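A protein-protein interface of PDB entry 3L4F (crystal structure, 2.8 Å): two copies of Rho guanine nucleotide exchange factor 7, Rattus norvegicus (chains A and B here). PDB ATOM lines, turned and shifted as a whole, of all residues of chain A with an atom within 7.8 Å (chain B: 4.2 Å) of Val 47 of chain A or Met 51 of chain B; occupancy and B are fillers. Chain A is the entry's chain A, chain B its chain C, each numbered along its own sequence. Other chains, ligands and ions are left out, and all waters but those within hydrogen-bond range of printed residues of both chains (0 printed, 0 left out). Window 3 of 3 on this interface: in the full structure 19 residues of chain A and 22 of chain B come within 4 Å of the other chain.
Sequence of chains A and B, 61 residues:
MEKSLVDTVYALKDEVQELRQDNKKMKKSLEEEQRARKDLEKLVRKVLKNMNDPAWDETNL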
ATOM      1  N   LEU A  40      15.944   9.352  -4.963  1.00  0.00           N
ATOM      2  CA  LEU A  40      15.616   8.070  -4.345  1.00  0.00           C
ATOM      3  C   LEU A  40      16.030   8.175  -2.884  1.00  0.00           C
ATOM      4  O   LEU A  40      15.445   7.528  -2.025  1.00  0.00           O
ATOM      5  CB  LEU A  40      16.390   6.907  -4.982  1.00  0.00           C
ATOM      6  CG  LEU A  40      15.648   5.565  -5.136  1.00  0.00           C
ATOM      7  CD1 LEU A  40      16.671   4.455  -5.071  1.00  0.00           C
ATOM      8  CD2 LEU A  40      14.585   5.348  -4.058  1.00  0.00           C
ATOM      9  N   GLU A  41      17.048   8.989  -2.604  1.00  0.00           N
ATOM     10  CA  GLU A  41      17.511   9.142  -1.227  1.00  0.00           C
ATOM     11  C   GLU A  41      16.465   9.893  -0.429  1.00  0.00           C
ATOM     12  O   GLU A  41      16.249   9.601   0.737  1.00  0.00           O
ATOM     13  CB  GLU A  41      18.857   9.861  -1.184  1.00  0.00           C
ATOM     14  CG  GLU A  41      19.962   9.068  -1.864  1.00  0.00           C
ATOM     15  CD  GLU A  41      21.311   9.733  -1.771  1.00  0.00           C
ATOM     16  OE1 GLU A  41      22.297   9.133  -2.253  1.00  0.00           O
ATOM     17  OE2 GLU A  41      21.384  10.849  -1.219  1.00  0.00           O
ATOM     18  N   LYS A  42      15.804  10.849  -1.077  1.00  0.00           N
ATOM     19  CA  LYS A  42      14.742  11.608  -0.446  1.00  0.00           C
ATOM     20  C   LYS A  42      13.563  10.682  -0.123  1.00  0.00           C
ATOM     21  O   LYS A  42      12.869  10.882   0.876  1.00  0.00           O
ATOM     22  CB  LYS A  42      14.291  12.755  -1.358  1.00  0.00           C
ATOM     23  CG  LYS A  42      15.305  13.883  -1.394  1.00  0.00           C
ATOM     24  CD  LYS A  42      14.992  14.930  -2.433  1.00  0.00           C
ATOM     25  CE  LYS A  42      16.202  15.855  -2.624  1.00  0.00           C
ATOM     26  NZ  LYS A  42      16.105  16.708  -3.849  1.00  0.00           N
ATOM     27  N   LEU A  43      13.317   9.684  -0.964  1.00  0.00           N
ATOM     28  CA  LEU A  43      12.235   8.743  -0.671  1.00  0.00           C
ATOM     29  C   LEU A  43      12.660   7.950   0.557  1.00  0.00           C
ATOM     30  O   LEU A  43      11.947   7.905   1.562  1.00  0.00           O
ATOM     31  CB  LEU A  43      12.004   7.769  -1.833  1.00  0.00           C
ATOM     32  CG  LEU A  43      10.782   8.002  -2.715  1.00  0.00           C
ATOM     33  CD1 LEU A  43      10.909   9.339  -3.443  1.00  0.00           C
ATOM     34  CD2 LEU A  43      10.668   6.857  -3.710  1.00  0.00           C
ATOM     35  N   VAL A  44      13.832   7.323   0.457  1.00  0.00           N
ATOM     36  CA  VAL A  44      14.393   6.523   1.541  1.00  0.00           C
ATOM     37  C   VAL A  44      14.396   7.328   2.839  1.00  0.00           C
ATOM     38  O   VAL A  44      14.003   6.829   3.897  1.00  0.00           O
ATOM     39  CB  VAL A  44      15.846   6.088   1.216  1.00  0.00           C
ATOM     40  CG1 VAL A  44      16.459   5.343   2.400  1.00  0.00           C
ATOM     41  CG2 VAL A  44      15.855   5.206  -0.015  1.00  0.00           C
ATOM     42  N   ARG A  45      14.833   8.582   2.734  1.00  0.00           N
ATOM     43  CA  ARG A  45      14.906   9.495   3.868  1.00  0.00           C
ATOM     44  C   ARG A  45      13.525   9.715   4.499  1.00  0.00           C
ATOM     45  O   ARG A  45      13.378   9.731   5.728  1.00  0.00           O
ATOM     46  CB  ARG A  45      15.474  10.837   3.405  1.00  0.00           C
ATOM     47  CG  ARG A  45      16.180  11.635   4.491  1.00  0.00           C
ATOM     48  CD  ARG A  45      16.519  13.039   4.005  1.00  0.00           C
ATOM     49  NE  ARG A  45      17.457  13.046   2.884  1.00  0.00           N
ATOM     50  CZ  ARG A  45      17.792  14.138   2.200  1.00  0.00           C
ATOM     51  NH1 ARG A  45      17.261  15.314   2.518  1.00  0.00           N
ATOM     52  NH2 ARG A  45      18.662  14.059   1.202  1.00  0.00           N
ATOM     53  N   LYS A  46      12.511   9.890   3.657  1.00  0.00           N
ATOM     54  CA  LYS A  46      11.166  10.124   4.151  1.00  0.00           C
ATOM     55  C   LYS A  46      10.479   8.815   4.516  1.00  0.00           C
ATOM     56  O   LYS A  46       9.479   8.804   5.230  1.00  0.00           O
ATOM     57  CB  LYS A  46      10.351  10.904   3.115  1.00  0.00           C
ATOM     58  CG  LYS A  46       9.240  10.120   2.436  1.00  0.00           C
ATOM     59  CD  LYS A  46       8.389  11.025   1.544  1.00  0.00           C
ATOM     60  CE  LYS A  46       7.476  11.948   2.349  1.00  0.00           C
ATOM     61  NZ  LYS A  46       8.217  12.867   3.261  1.00  0.00           N
ATOM     62  N   VAL A  47      11.008   7.706   4.024  1.00  0.00           N
ATOM     63  CA  VAL A  47      10.437   6.414   4.376  1.00  0.00           C
ATOM     64  C   VAL A  47      10.882   6.168   5.805  1.00  0.00           C
ATOM     65  O   VAL A  47      10.223   5.465   6.565  1.00  0.00           O
ATOM     66  CB  VAL A  47      10.968   5.288   3.463  1.00  0.00           C
ATOM     67  CG1 VAL A  47      10.790   3.918   4.134  1.00  0.00           C
ATOM     68  CG2 VAL A  47      10.222   5.328   2.144  1.00  0.00           C
ATOM     69  N   LEU A  48      12.011   6.776   6.155  1.00  0.00           N
ATOM     70  CA  LEU A  48      12.590   6.665   7.491  1.00  0.00           C
ATOM     71  C   LEU A  48      11.900   7.575   8.495  1.00  0.00           C
ATOM     72  O   LEU A  48      11.582   7.146   9.601  1.00  0.00           O
ATOM     73  CB  LEU A  48      14.083   6.998   7.453  1.00  0.00           C
ATOM     74  CG  LEU A  48      14.978   5.956   6.779  1.00  0.00           C
ATOM     75  CD1 LEU A  48      16.365   6.537   6.587  1.00  0.00           C
ATOM     76  CD2 LEU A  48      15.019   4.684   7.626  1.00  0.00           C
ATOM     77  N   LYS A  49      11.679   8.831   8.115  1.00  0.00           N
ATOM     78  CA  LYS A  49      11.017   9.782   9.004  1.00  0.00           C
ATOM     79  C   LYS A  49       9.672   9.227   9.466  1.00  0.00           C
ATOM     80  O   LYS A  49       9.217   9.522  10.563  1.00  0.00           O
ATOM     81  CB  LYS A  49      10.815  11.125   8.296  1.00  0.00           C
ATOM     82  CG  LYS A  49      10.277  12.240   9.191  1.00  0.00           C
ATOM     83  CD  LYS A  49      10.251  13.570   8.450  1.00  0.00           C
ATOM     84  CE  LYS A  49       9.824  14.717   9.344  1.00  0.00           C
ATOM     85  NZ  LYS A  49       9.956  16.015   8.623  1.00  0.00           N
ATOM     86  N   ASN A  50       9.056   8.403   8.627  1.00  0.00           N
ATOM     87  CA  ASN A  50       7.765   7.810   8.950  1.00  0.00           C
ATOM     88  C   ASN A  50       7.900   6.498   9.743  1.00  0.00           C
ATOM     89  O   ASN A  50       6.980   6.087  10.450  1.00  0.00           O
ATOM     90  CB  ASN A  50       6.975   7.592   7.656  1.00  0.00           C
ATOM     91  CG  ASN A  50       6.894   8.858   6.802  1.00  0.00           C
ATOM     92  OD1 ASN A  50       6.294   8.861   5.725  1.00  0.00           O
ATOM     93  ND2 ASN A  50       7.503   9.937   7.282  1.00  0.00           N
ATOM     94  N   MET A  51       9.044   5.836   9.613  1.00  0.00           N
ATOM     95  CA  MET A  51       9.289   4.605  10.356  1.00  0.00           C
ATOM     96  C   MET A  51       9.316   5.032  11.818  1.00  0.00           C
ATOM     97  O   MET A  51       8.794   4.340  12.686  1.00  0.00           O
ATOM     98  CB  MET A  51      10.657   4.013   9.990  1.00  0.00           C
ATOM     99  CG  MET A  51      10.825   3.601   8.533  1.00  0.00           C
ATOM    100  SD  MET A  51      10.244   1.927   8.160  1.00  0.00           S
ATOM    101  CE  MET A  51      11.723   0.975   8.566  1.00  0.00           C
ATOM    102  N   ASN A  52       9.917   6.197  12.058  1.00  0.00           N
ATOM    103  CA  ASN A  52      10.076   6.760  13.393  1.00  0.00           C
ATOM    104  C   ASN A  52       8.825   7.426  13.942  1.00  0.00           C
ATOM    105  O   ASN A  52       8.199   6.886  14.845  1.00  0.00           O
ATOM    106  CB  ASN A  52      11.238   7.761  13.393  1.00  0.00           C
ATOM    107  CG  ASN A  52      11.309   8.577  14.675  1.00  0.00           C
ATOM    108  OD1 ASN A  52      11.300   8.030  15.781  1.00  0.00           O
ATOM    109  ND2 ASN A  52      11.387   9.896  14.530  1.00  0.00           N
ATOM    110  N   ASP A  53       8.488   8.604  13.412  1.00  0.00           N
ATOM    111  CA  ASP A  53       7.302   9.354  13.824  1.00  0.00           C
ATOM    112  C   ASP A  53       6.297   9.417  12.657  1.00  0.00           C
ATOM    113  O   ASP A  53       6.270  10.386  11.893  1.00  0.00           O
ATOM    114  CB  ASP A  53       7.690  10.773  14.252  1.00  0.00           C
ATOM    115  CG  ASP A  53       6.737  11.347  15.284  1.00  0.00           C
ATOM    116  OD1 ASP A  53       5.513  11.388  15.021  1.00  0.00           O
ATOM    117  OD2 ASP A  53       7.213  11.751  16.363  1.00  0.00           O
ATOM    118  N   VAL B  47       8.614  -0.828   0.489  1.00  0.00           N
ATOM    119  CA  VAL B  47       8.607  -0.287   1.839  1.00  0.00           C
ATOM    120  C   VAL B  47       8.441   1.226   1.745  1.00  0.00           C
ATOM    121  O   VAL B  47       9.171   1.988   2.379  1.00  0.00           O
ATOM    122  CB  VAL B  47       9.926  -0.619   2.565  1.00  0.00           C
ATOM    123  CG1 VAL B  47      10.020  -2.113   2.793  1.00  0.00           C
ATOM    124  CG2 VAL B  47      11.114  -0.144   1.738  1.00  0.00           C
ATOM    125  N   LEU B  48       7.486   1.652   0.928  1.00  0.00           N
ATOM    126  CA  LEU B  48       7.212   3.069   0.749  1.00  0.00           C
ATOM    127  C   LEU B  48       5.718   3.304   0.726  1.00  0.00           C
ATOM    128  O   LEU B  48       5.203   4.145   1.461  1.00  0.00           O
ATOM    129  CB  LEU B  48       7.810   3.590  -0.557  1.00  0.00           C
ATOM    130  CG  LEU B  48       7.520   5.079  -0.788  1.00  0.00           C
ATOM    131  CD1 LEU B  48       8.767   5.913  -0.523  1.00  0.00           C
ATOM    132  CD2 LEU B  48       7.042   5.288  -2.220  1.00  0.00           C
ATOM    133  N   LYS B  49       5.028   2.561  -0.131  1.00  0.00           N
ATOM    134  CA  LYS B  49       3.584   2.681  -0.258  1.00  0.00           C
ATOM    135  C   LYS B  49       2.916   1.681   0.678  1.00  0.00           C
ATOM    136  O   LYS B  49       1.791   1.892   1.136  1.00  0.00           O
ATOM    137  CB  LYS B  49       3.162   2.411  -1.702  1.00  0.00           C
ATOM    138  CG  LYS B  49       1.697   2.678  -1.984  1.00  0.00           C
ATOM    139  CD  LYS B  49       1.413   2.572  -3.467  1.00  0.00           C
ATOM    140  CE  LYS B  49       0.031   3.084  -3.787  1.00  0.00           C
ATOM    141  NZ  LYS B  49      -0.149   3.155  -5.252  1.00  0.00           N
ATOM    142  N   ASN B  50       3.623   0.590   0.954  1.00  0.00           N
ATOM    143  CA  ASN B  50       3.115  -0.443   1.843  1.00  0.00           C
ATOM    144  C   ASN B  50       3.240   0.025   3.283  1.00  0.00           C
ATOM    145  O   ASN B  50       2.320   0.645   3.806  1.00  0.00           O
ATOM    146  CB  ASN B  50       3.885  -1.749   1.643  1.00  0.00           C
ATOM    147  CG  ASN B  50       3.541  -2.427   0.331  1.00  0.00           C
ATOM    148  OD1 ASN B  50       3.543  -1.796  -0.726  1.00  0.00           O
ATOM    149  ND2 ASN B  50       3.244  -3.722   0.392  1.00  0.00           N
ATOM    150  N   MET B  51       4.380  -0.246   3.915  1.00  0.00           N
ATOM    151  CA  MET B  51       4.591   0.150   5.306  1.00  0.00           C
ATOM    152  C   MET B  51       3.365  -0.149   6.162  1.00  0.00           C
ATOM    153  O   MET B  51       3.288  -1.200   6.805  1.00  0.00           O
ATOM    154  CB  MET B  51       4.956   1.642   5.396  1.00  0.00           C
ATOM    155  CG  MET B  51       6.372   1.973   4.941  1.00  0.00           C
ATOM    156  SD  MET B  51       6.993   3.497   5.667  1.00  0.00           S
ATOM    157  CE  MET B  51       7.497   4.446   4.189  1.00  0.00           C
ATOM    158  N   ASN B  52       2.416   0.782   6.170  1.00  0.00           N
ATOM    159  CA  ASN B  52       1.173   0.644   6.925  1.00  0.00           C
ATOM    160  C   ASN B  52       0.103   1.447   6.167  1.00  0.00           C
ATOM    161  O   ASN B  52      -0.308   2.499   6.547  1.00  0.00           O
ATOM    162  CB  ASN B  52       1.345   1.165   8.339  1.00  0.00           C
ATOM    163  CG  ASN B  52       2.304   0.315   9.160  1.00  0.00           C
ATOM    164  OD1 ASN B  52       2.110  -0.892   9.284  1.00  0.00           O
ATOM    165  ND2 ASN B  52       3.363   0.928   9.682  1.00  0.00           N
ATOM    166  N   ASP B  53      -0.266   0.910   5.029  1.00  0.00           N
ATOM    167  CA  ASP B  53      -1.309   1.477   4.191  1.00  0.00           C
ATOM    168  C   ASP B  53      -1.777   0.455   3.177  1.00  0.00           C
ATOM    169  O   ASP B  53      -1.810   0.835   1.989  1.00  0.00           O
ATOM    170  CB  ASP B  53      -0.813   2.708   3.451  1.00  0.00           C
ATOM    171  CG  ASP B  53      -1.079   3.986   4.198  1.00  0.00           C
ATOM    172  OD1 ASP B  53      -2.272   4.344   4.336  1.00  0.00           O
ATOM    173  OD2 ASP B  53      -0.104   4.647   4.618  1.00  0.00           O
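Val 47 of chain B touches its own counterpart, Val 47 of chain A. Val 47 of chain A touches Leu 48 of chain B, but with the chains exchanged Leu 48 of chain A does not touch Val 47 of chain B (6.7 Å). Val 47 of chain A touches Met 51 of chain B, but with the chains exchanged Met 51 of chain A does not touch Val 47 of chain B (5.9 Å). Positions printed for both chains: 47, 48, 49, 50, 51, 52 and 53.
Glu 41 of chain A touches none of the printed residues of chain B. Lys 42 of chain A touches none of the printed residues of chain B. Printed residues of chain B within 4 Å of Leu 43 of chain A: Leu 48. Val 47 of chain A touches just these residues of chain B: Val 47, Leu 48 and Met 51. Printed residues of chain A within 4 Å of Val 47 of chain B: Val 47 (3.1 Å). Of the printed residues of chain A, Leu 48 of chain B touches Leu 43 and Val 47. Printed residues of chain A within 4 Å of Met 51 of chain B: Val 47 (3.3 Å). The nearest printed residue of chain A that does not touch Leu 48 of chain B is Lys 46 of chain A (5.2 Å).
Of the 7 printed residues of chain B, 3 touch a printed residue of chain A. Hydrophobic or aromatic side chains of chain B that line the printed part of chain A: Leu 48 and Met 51. Along chain B the printed residues that touch a printed residue of chain A span positions 47 to 51. Printed residues of chain A that touch a printed residue of chain B: Leu 43 and Val 47. Among the printed residues, no Asp or Glu carboxylate lies within 4 Å of a Lys or Arg side-chain nitrogen of the other chain.
Leu 43 of chain A touches Leu 48 of chain B. Val 47 of chain B touches Val 47 of chain A (O to CG1, 3.1 Å). Val 47 of chain A touches Leu 48 of chain B. CE of Met 51 of chain B touches CG1 of Val 47 of chain A, 3.3 Å away.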
